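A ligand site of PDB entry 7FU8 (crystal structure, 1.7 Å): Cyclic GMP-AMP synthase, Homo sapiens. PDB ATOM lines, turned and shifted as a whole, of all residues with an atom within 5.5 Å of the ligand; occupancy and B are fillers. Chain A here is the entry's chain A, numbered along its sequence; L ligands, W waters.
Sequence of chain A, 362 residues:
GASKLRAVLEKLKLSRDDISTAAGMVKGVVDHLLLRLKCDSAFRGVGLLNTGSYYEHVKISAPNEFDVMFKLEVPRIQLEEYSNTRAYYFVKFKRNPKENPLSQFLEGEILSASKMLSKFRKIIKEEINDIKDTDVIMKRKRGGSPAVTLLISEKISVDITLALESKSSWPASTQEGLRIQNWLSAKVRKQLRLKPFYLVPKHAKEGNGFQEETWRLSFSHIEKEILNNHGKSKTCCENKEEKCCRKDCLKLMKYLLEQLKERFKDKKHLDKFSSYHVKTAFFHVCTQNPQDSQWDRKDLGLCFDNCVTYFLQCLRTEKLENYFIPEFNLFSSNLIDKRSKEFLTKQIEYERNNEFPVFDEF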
ATOM      1  N   ARG A  86      15.985 -32.818   1.792  1.00  0.00           N
ATOM      2  CA  ARG A  86      16.131 -32.730   0.337  1.00  0.00           C
ATOM      3  C   ARG A  86      17.553 -33.046  -0.155  1.00  0.00           C
ATOM      4  O   ARG A  86      17.720 -33.578  -1.261  1.00  0.00           O
ATOM      5  CB  ARG A  86      15.684 -31.349  -0.168  1.00  0.00           C
ATOM      6  CG  ARG A  86      14.179 -31.080  -0.034  1.00  0.00           C
ATOM      7  CD  ARG A  86      13.332 -32.143  -0.734  1.00  0.00           C
ATOM      8  NE  ARG A  86      11.904 -31.836  -0.647  1.00  0.00           N
ATOM      9  CZ  ARG A  86      11.044 -32.401   0.196  1.00  0.00           C
ATOM     10  NH1 ARG A  86      11.450 -33.334   1.059  1.00  0.00           N
ATOM     11  NH2 ARG A  86       9.759 -32.041   0.187  1.00  0.00           N
ATOM     12  N   ALA A  87      18.588 -32.756   0.647  1.00  0.00           N
ATOM     13  CA  ALA A  87      19.963 -33.005   0.240  1.00  0.00           C
ATOM     14  C   ALA A  87      20.627 -34.211   0.890  1.00  0.00           C
ATOM     15  O   ALA A  87      21.650 -34.689   0.383  1.00  0.00           O
ATOM     16  CB  ALA A  87      20.841 -31.773   0.536  1.00  0.00           C
ATOM     17  N   TYR A  88      20.096 -34.703   2.022  1.00  0.00           N
ATOM     18  CA  TYR A  88      20.780 -35.678   2.865  1.00  0.00           C
ATOM     19  C   TYR A  88      19.987 -36.986   2.889  1.00  0.00           C
ATOM     20  O   TYR A  88      18.769 -36.977   3.033  1.00  0.00           O
ATOM     21  CB  TYR A  88      20.949 -35.166   4.304  1.00  0.00           C
ATOM     22  CG  TYR A  88      21.793 -33.932   4.342  1.00  0.00           C
ATOM     23  CD1 TYR A  88      23.174 -34.020   4.289  1.00  0.00           C
ATOM     24  CD2 TYR A  88      21.211 -32.671   4.369  1.00  0.00           C
ATOM     25  CE1 TYR A  88      23.963 -32.872   4.286  1.00  0.00           C
ATOM     26  CE2 TYR A  88      21.982 -31.532   4.377  1.00  0.00           C
ATOM     27  CZ  TYR A  88      23.361 -31.647   4.343  1.00  0.00           C
ATOM     28  OH  TYR A  88      24.143 -30.523   4.327  1.00  0.00           O
ATOM     29  N   GLU A 206      28.258 -30.090   9.986  1.00  0.00           N
ATOM     30  CA  GLU A 206      27.192 -29.970   9.009  1.00  0.00           C
ATOM     31  C   GLU A 206      26.006 -30.799   9.486  1.00  0.00           C
ATOM     32  O   GLU A 206      26.180 -31.941   9.922  1.00  0.00           O
ATOM     33  CB  GLU A 206      27.678 -30.440   7.640  1.00  0.00           C
ATOM     34  CG  GLU A 206      26.739 -30.271   6.462  1.00  0.00           C
ATOM     35  CD  GLU A 206      27.342 -30.846   5.179  1.00  0.00           C
ATOM     36  OE1 GLU A 206      28.545 -31.204   5.181  1.00  0.00           O
ATOM     37  OE2 GLU A 206      26.618 -30.952   4.164  1.00  0.00           O
ATOM     38  N   ARG A 216      25.338 -36.762   1.498  1.00  0.00           N
ATOM     39  CA  ARG A 216      24.894 -35.568   0.801  1.00  0.00           C
ATOM     40  C   ARG A 216      25.077 -35.736  -0.707  1.00  0.00           C
ATOM     41  O   ARG A 216      26.102 -36.252  -1.159  1.00  0.00           O
ATOM     42  CB  ARG A 216      25.684 -34.353   1.282  1.00  0.00           C
ATOM     43  CG  ARG A 216      25.119 -33.057   0.812  1.00  0.00           C
ATOM     44  CD  ARG A 216      25.991 -31.914   1.261  1.00  0.00           C
ATOM     45  NE  ARG A 216      27.203 -31.876   0.456  1.00  0.00           N
ATOM     46  CZ  ARG A 216      28.438 -31.854   0.947  1.00  0.00           C
ATOM     47  NH1 ARG A 216      29.466 -31.820   0.106  1.00  0.00           N
ATOM     48  NH2 ARG A 216      28.657 -31.850   2.257  1.00  0.00           N
ATOM     49  N   LEU A 217      24.085 -35.295  -1.474  1.00  0.00           N
ATOM     50  CA  LEU A 217      24.207 -35.352  -2.925  1.00  0.00           C
ATOM     51  C   LEU A 217      25.313 -34.420  -3.413  1.00  0.00           C
ATOM     52  O   LEU A 217      25.601 -33.385  -2.811  1.00  0.00           O
ATOM     53  CB  LEU A 217      22.883 -34.960  -3.597  1.00  0.00           C
ATOM     54  CG  LEU A 217      21.728 -35.935  -3.371  1.00  0.00           C
ATOM     55  CD1 LEU A 217      20.393 -35.329  -3.821  1.00  0.00           C
ATOM     56  CD2 LEU A 217      22.028 -37.219  -4.123  1.00  0.00           C
ATOM     57  N   SER A 218      25.968 -34.833  -4.502  1.00  0.00           N
ATOM     58  CA  SER A 218      27.086 -34.092  -5.071  1.00  0.00           C
ATOM     59  C   SER A 218      27.013 -34.170  -6.582  1.00  0.00           C
ATOM     60  O   SER A 218      26.874 -35.265  -7.148  1.00  0.00           O
ATOM     61  CB  SER A 218      28.422 -34.657  -4.576  1.00  0.00           C
ATOM     62  OG  SER A 218      29.504 -34.110  -5.304  1.00  0.00           O
ATOM     63  N   PHE A 219      27.126 -33.024  -7.251  1.00  0.00           N
ATOM     64  CA  PHE A 219      27.027 -32.949  -8.709  1.00  0.00           C
ATOM     65  C   PHE A 219      28.237 -32.234  -9.293  1.00  0.00           C
ATOM     66  O   PHE A 219      28.127 -31.450 -10.249  1.00  0.00           O
ATOM     67  CB  PHE A 219      25.745 -32.242  -9.143  1.00  0.00           C
ATOM     68  CG  PHE A 219      24.480 -32.941  -8.696  1.00  0.00           C
ATOM     69  CD1 PHE A 219      23.970 -33.999  -9.413  1.00  0.00           C
ATOM     70  CD2 PHE A 219      23.826 -32.542  -7.536  1.00  0.00           C
ATOM     71  CE1 PHE A 219      22.831 -34.650  -8.983  1.00  0.00           C
ATOM     72  CE2 PHE A 219      22.669 -33.192  -7.097  1.00  0.00           C
ATOM     73  CZ  PHE A 219      22.172 -34.253  -7.831  1.00  0.00           C
ATOM     74  N   SER A 220      29.433 -32.493  -8.754  1.00  0.00           N
ATOM     75  CA  SER A 220      30.588 -31.716  -9.179  1.00  0.00           C
ATOM     76  C   SER A 220      31.001 -32.064 -10.614  1.00  0.00           C
ATOM     77  O   SER A 220      31.558 -31.217 -11.316  1.00  0.00           O
ATOM     78  CB  SER A 220      31.766 -31.934  -8.219  1.00  0.00           C
ATOM     79  OG  SER A 220      32.272 -33.237  -8.357  1.00  0.00           O
ATOM     80  N   GLU A 223      28.808 -29.636 -12.698  1.00  0.00           N
ATOM     81  CA  GLU A 223      29.438 -28.325 -12.690  1.00  0.00           C
ATOM     82  C   GLU A 223      30.590 -28.264 -13.690  1.00  0.00           C
ATOM     83  O   GLU A 223      30.695 -27.322 -14.483  1.00  0.00           O
ATOM     84  CB  GLU A 223      29.933 -27.997 -11.281  1.00  0.00           C
ATOM     85  CG  GLU A 223      30.871 -26.809 -11.253  1.00  0.00           C
ATOM     86  CD  GLU A 223      31.643 -26.717  -9.949  1.00  0.00           C
ATOM     87  OE1 GLU A 223      31.040 -26.942  -8.887  1.00  0.00           O
ATOM     88  OE2 GLU A 223      32.867 -26.437 -10.001  1.00  0.00           O
ATOM     89  N   TYR A 276      31.227 -22.685  -2.725  1.00  0.00           N
ATOM     90  CA  TYR A 276      29.938 -23.281  -3.049  1.00  0.00           C
ATOM     91  C   TYR A 276      28.861 -22.203  -3.236  1.00  0.00           C
ATOM     92  O   TYR A 276      28.091 -22.237  -4.190  1.00  0.00           O
ATOM     93  CB  TYR A 276      29.584 -24.267  -1.940  1.00  0.00           C
ATOM     94  CG  TYR A 276      28.170 -24.773  -1.907  1.00  0.00           C
ATOM     95  CD1 TYR A 276      27.582 -25.293  -3.037  1.00  0.00           C
ATOM     96  CD2 TYR A 276      27.446 -24.763  -0.711  1.00  0.00           C
ATOM     97  CE1 TYR A 276      26.292 -25.783  -3.023  1.00  0.00           C
ATOM     98  CE2 TYR A 276      26.142 -25.250  -0.679  1.00  0.00           C
ATOM     99  CZ  TYR A 276      25.571 -25.756  -1.845  1.00  0.00           C
ATOM    100  OH  TYR A 276      24.290 -26.255  -1.878  1.00  0.00           O
ATOM    101  N   LYS A 279      29.715 -20.077  -6.424  1.00  0.00           N
ATOM    102  CA  LYS A 279      29.443 -20.874  -7.624  1.00  0.00           C
ATOM    103  C   LYS A 279      27.945 -20.973  -7.898  1.00  0.00           C
ATOM    104  O   LYS A 279      27.501 -20.824  -9.036  1.00  0.00           O
ATOM    105  CB  LYS A 279      30.055 -22.272  -7.491  1.00  0.00           C
ATOM    106  CG  LYS A 279      31.571 -22.306  -7.682  1.00  0.00           C
ATOM    107  CD  LYS A 279      32.155 -23.740  -7.698  1.00  0.00           C
ATOM    108  CE  LYS A 279      32.074 -24.409  -6.337  1.00  0.00           C
ATOM    109  NZ  LYS A 279      32.156 -25.903  -6.425  1.00  0.00           N
ATOM    110  N   THR A 280      27.156 -21.238  -6.849  1.00  0.00           N
ATOM    111  CA  THR A 280      25.706 -21.340  -7.020  1.00  0.00           C
ATOM    112  C   THR A 280      25.128 -20.047  -7.587  1.00  0.00           C
ATOM    113  O   THR A 280      24.349 -20.076  -8.561  1.00  0.00           O
ATOM    114  CB  THR A 280      25.050 -21.691  -5.670  1.00  0.00           C
ATOM    115  OG1 THR A 280      25.583 -22.928  -5.200  1.00  0.00           O
ATOM    116  CG2 THR A 280      23.558 -21.822  -5.813  1.00  0.00           C
ATOM    117  N   PHE A 283      26.056 -19.552 -11.337  1.00  0.00           N
ATOM    118  CA  PHE A 283      25.272 -20.353 -12.263  1.00  0.00           C
ATOM    119  C   PHE A 283      23.871 -19.782 -12.432  1.00  0.00           C
ATOM    120  O   PHE A 283      23.300 -19.829 -13.525  1.00  0.00           O
ATOM    121  CB  PHE A 283      25.236 -21.812 -11.788  1.00  0.00           C
ATOM    122  CG  PHE A 283      26.406 -22.638 -12.297  1.00  0.00           C
ATOM    123  CD1 PHE A 283      27.663 -22.512 -11.718  1.00  0.00           C
ATOM    124  CD2 PHE A 283      26.254 -23.517 -13.361  1.00  0.00           C
ATOM    125  CE1 PHE A 283      28.761 -23.234 -12.197  1.00  0.00           C
ATOM    126  CE2 PHE A 283      27.345 -24.267 -13.829  1.00  0.00           C
ATOM    127  CZ  PHE A 283      28.591 -24.122 -13.250  1.00  0.00           C
ATOM    128  N   ASN A 322      19.840 -23.738  -4.113  1.00  0.00           N
ATOM    129  CA  ASN A 322      20.757 -24.696  -4.704  1.00  0.00           C
ATOM    130  C   ASN A 322      20.402 -24.881  -6.174  1.00  0.00           C
ATOM    131  O   ASN A 322      19.224 -24.944  -6.545  1.00  0.00           O
ATOM    132  CB  ASN A 322      20.705 -26.027  -3.969  1.00  0.00           C
ATOM    133  CG  ASN A 322      21.660 -27.061  -4.547  1.00  0.00           C
ATOM    134  OD1 ASN A 322      21.327 -27.784  -5.485  1.00  0.00           O
ATOM    135  ND2 ASN A 322      22.834 -27.164  -3.947  1.00  0.00           N
ATOM    136  N   TYR A 323      21.422 -24.954  -7.028  1.00  0.00           N
ATOM    137  CA  TYR A 323      21.203 -25.009  -8.473  1.00  0.00           C
ATOM    138  C   TYR A 323      20.519 -26.299  -8.917  1.00  0.00           C
ATOM    139  O   TYR A 323      19.778 -26.307  -9.904  1.00  0.00           O
ATOM    140  CB  TYR A 323      22.537 -24.828  -9.192  1.00  0.00           C
ATOM    141  CG  TYR A 323      22.383 -24.348 -10.618  1.00  0.00           C
ATOM    142  CD1 TYR A 323      21.886 -23.071 -10.876  1.00  0.00           C
ATOM    143  CD2 TYR A 323      22.715 -25.167 -11.693  1.00  0.00           C
ATOM    144  CE1 TYR A 323      21.743 -22.611 -12.164  1.00  0.00           C
ATOM    145  CE2 TYR A 323      22.581 -24.703 -13.009  1.00  0.00           C
ATOM    146  CZ  TYR A 323      22.089 -23.438 -13.233  1.00  0.00           C
ATOM    147  OH  TYR A 323      21.945 -22.968 -14.523  1.00  0.00           O
ATOM    148  N   PHE A 324      20.737 -27.391  -8.184  1.00  0.00           N
ATOM    149  CA  PHE A 324      20.161 -28.688  -8.518  1.00  0.00           C
ATOM    150  C   PHE A 324      18.896 -28.994  -7.742  1.00  0.00           C
ATOM    151  O   PHE A 324      18.027 -29.708  -8.250  1.00  0.00           O
ATOM    152  CB  PHE A 324      21.203 -29.781  -8.288  1.00  0.00           C
ATOM    153  CG  PHE A 324      22.454 -29.574  -9.088  1.00  0.00           C
ATOM    154  CD1 PHE A 324      23.502 -28.803  -8.580  1.00  0.00           C
ATOM    155  CD2 PHE A 324      22.582 -30.107 -10.369  1.00  0.00           C
ATOM    156  CE1 PHE A 324      24.657 -28.572  -9.328  1.00  0.00           C
ATOM    157  CE2 PHE A 324      23.742 -29.888 -11.128  1.00  0.00           C
ATOM    158  CZ  PHE A 324      24.777 -29.125 -10.600  1.00  0.00           C
ATOM    159  N   ILE A 325      18.783 -28.474  -6.522  1.00  0.00           N
ATOM    160  CA  ILE A 325      17.694 -28.842  -5.632  1.00  0.00           C
ATOM    161  C   ILE A 325      17.083 -27.524  -5.160  1.00  0.00           C
ATOM    162  O   ILE A 325      17.519 -26.959  -4.139  1.00  0.00           O
ATOM    163  CB  ILE A 325      18.200 -29.746  -4.494  1.00  0.00           C
ATOM    164  CG1 ILE A 325      18.761 -31.050  -5.070  1.00  0.00           C
ATOM    165  CG2 ILE A 325      17.095 -30.087  -3.522  1.00  0.00           C
ATOM    166  CD1 ILE A 325      19.491 -31.899  -4.045  1.00  0.00           C
ATOM    167  N   PHE A 328      16.263 -26.264  -1.518  1.00  0.00           N
ATOM    168  CA  PHE A 328      17.290 -26.090  -0.497  1.00  0.00           C
ATOM    169  C   PHE A 328      17.826 -24.673  -0.575  1.00  0.00           C
ATOM    170  O   PHE A 328      18.439 -24.299  -1.579  1.00  0.00           O
ATOM    171  CB  PHE A 328      18.400 -27.120  -0.659  1.00  0.00           C
ATOM    172  CG  PHE A 328      19.331 -27.197   0.520  1.00  0.00           C
ATOM    173  CD1 PHE A 328      20.309 -26.225   0.712  1.00  0.00           C
ATOM    174  CD2 PHE A 328      19.234 -28.226   1.425  1.00  0.00           C
ATOM    175  CE1 PHE A 328      21.154 -26.278   1.802  1.00  0.00           C
ATOM    176  CE2 PHE A 328      20.078 -28.279   2.515  1.00  0.00           C
ATOM    177  CZ  PHE A 328      21.047 -27.302   2.687  1.00  0.00           C
ATOM    178  N   LEU A 330      20.430 -22.213   0.442  1.00  0.00           N
ATOM    179  CA  LEU A 330      21.765 -22.050   1.019  1.00  0.00           C
ATOM    180  C   LEU A 330      21.816 -20.931   2.045  1.00  0.00           C
ATOM    181  O   LEU A 330      22.637 -20.971   2.971  1.00  0.00           O
ATOM    182  CB  LEU A 330      22.802 -21.751  -0.068  1.00  0.00           C
ATOM    183  CG  LEU A 330      22.865 -22.666  -1.284  1.00  0.00           C
ATOM    184  CD1 LEU A 330      24.186 -22.446  -2.008  1.00  0.00           C
ATOM    185  CD2 LEU A 330      22.685 -24.067  -0.812  1.00  0.00           C
HETATM  186  C1  LIG L   1      27.597 -28.618  -1.038  1.00  0.00           C
HETATM  187  C2  LIG L   1      28.877 -28.394  -0.577  1.00  0.00           C
HETATM  188  C3  LIG L   1      28.168 -28.288   1.592  1.00  0.00           C
HETATM  189  C4  LIG L   1      25.334 -30.132  -4.988  1.00  0.00           C
HETATM  190  C5  LIG L   1      28.095 -29.140  -6.813  1.00  0.00           C
HETATM  191  C6  LIG L   1      28.249 -27.799  -7.313  1.00  0.00           C
HETATM  192  C7  LIG L   1      27.306 -26.830  -7.124  1.00  0.00           C
HETATM  193  C8  LIG L   1      25.964 -28.369  -5.902  1.00  0.00           C
HETATM  194  C9  LIG L   1      27.400 -25.420  -7.614  1.00  0.00           C
HETATM  195  C10 LIG L   1      26.527 -25.093  -8.798  1.00  0.00           C
HETATM  196  C11 LIG L   1      26.986 -25.720 -10.077  1.00  0.00           C
HETATM  197  C12 LIG L   1      23.590 -29.770  -2.237  1.00  0.00           C
HETATM  198  C13 LIG L   1      26.854 -28.495   1.222  1.00  0.00           C
HETATM  199  C14 LIG L   1      23.317 -30.496  -3.534  1.00  0.00           C
HETATM  200  C15 LIG L   1      24.880 -29.555  -1.778  1.00  0.00           C
HETATM  201  C16 LIG L   1      25.150 -28.892  -0.576  1.00  0.00           C
HETATM  202  C17 LIG L   1      24.072 -28.408   0.162  1.00  0.00           C
HETATM  203  C18 LIG L   1      22.783 -28.587  -0.273  1.00  0.00           C
HETATM  204  C19 LIG L   1      22.554 -29.253  -1.459  1.00  0.00           C
HETATM  205  C20 LIG L   1      26.548 -28.679  -0.123  1.00  0.00           C
HETATM  206  N1  LIG L   1      29.180 -28.221   0.716  1.00  0.00           N
HETATM  207  N2  LIG L   1      24.499 -30.993  -4.239  1.00  0.00           N
HETATM  208  N3  LIG L   1      26.504 -30.504  -5.493  1.00  0.00           N
HETATM  209  N4  LIG L   1      26.893 -29.330  -6.097  1.00  0.00           N
HETATM  210  N5  LIG L   1      26.157 -27.119  -6.409  1.00  0.00           N
HETATM  211  N6  LIG L   1      24.951 -28.834  -5.194  1.00  0.00           N
HETATM  212  O1  LIG L   1      28.896 -30.074  -6.930  1.00  0.00           O
HETATM  213 CL1  LIG L   1      20.903 -29.451  -1.976  1.00  0.00          CL
HETATM  214  O   HOH W   1      29.527 -31.427  -4.681  1.00  0.00           O
HETATM  215  O   HOH W   2      31.482 -29.005  -6.974  1.00  0.00           O
HETATM  216  O   HOH W   3      24.051 -25.027  -6.217  1.00  0.00           O
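Ala 87 touches the ligand (CB to CL1, 3.4 Å).
OE2 of Glu 206 touches C13 of the ligand, 3.8 Å away.
Arg 216 touches the ligand.
Ser 218 touches the ligand.
OE1 of Glu 223 touches C6 of the ligand (3.3 Å).
Tyr 276 touches the ligand.
Thr 280 touches the ligand (OG1 to C9, 3.9 Å).
Phe 283 touches the ligand (CD1 to C11, 3.7 Å).
Phe 324 touches the ligand (CE1 to N5, 3.6 Å).
Ile 325 touches the ligand (CD1 to CL1, 3.5 Å).
CE1 of Phe 328 touches C18 of the ligand, 3.5 Å away.
Of the 20 residues printed, 15 come within 4 Å of the ligand.
The backbone NH of Phe 219 lies within hydrogen-bond range of a nitrogen (N3) of the ligand, at 3.1 Å.
ND2 of Asn 322 is in hydrogen-bond range of N6 of the ligand (3.0 Å).
The backbone carbonyl oxygen (O) of Leu 217 lies within hydrogen-bond range of a nitrogen (N2) of the ligand.
The backbone NH of Ser 220 is in hydrogen-bond range of an oxygen (O1) of the ligand (3.1 Å).
The guanidinium group (NH2) of Arg 216 is in salt-bridge range of the side-chain carboxylate (OE2) of Glu 206 (2.9 Å).
OD1 of Asn 322 is in hydrogen-bond range of N of Ile 325, at 2.8 Å.
The backbone carbonyl oxygen (O) of Tyr 276 lies within hydrogen-bond range of the side-chain hydroxyl (OG1) of Thr 280 (2.8 Å).
The backbone NH (N) of Phe 324 sits at hydrogen-bond distance from the side-chain amide oxygen (OD1) of Asn 322.
The side-chain amide nitrogen (ND2) of Asn 322 lies within hydrogen-bond range of the side-chain hydroxyl (OH) of Tyr 276 (2.7 Å).
The side-chain carboxylate (OE1) of Glu 223 lies within salt-bridge range of the side-chain amino group (NZ) of Lys 279 (2.9 Å).
O of Ala 87 sits at hydrogen-bond distance from N of Leu 217 (3.1 Å).
The backbone carbonyl oxygen of Phe 328 sits at hydrogen-bond distance from the backbone NH of Asn 322 (2.9 Å).
Water W1 bridges an oxygen (O1) of the ligand (2.7 Å) and the side-chain hydroxyl of Ser 218 (2.8 Å).
Water W2 lies within hydrogen-bond range of an oxygen (O1) of the ligand (2.8 Å), the side-chain carboxylate of Glu 223 (2.8 Å) and the side-chain amino group of Lys 279 (3.2 Å).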
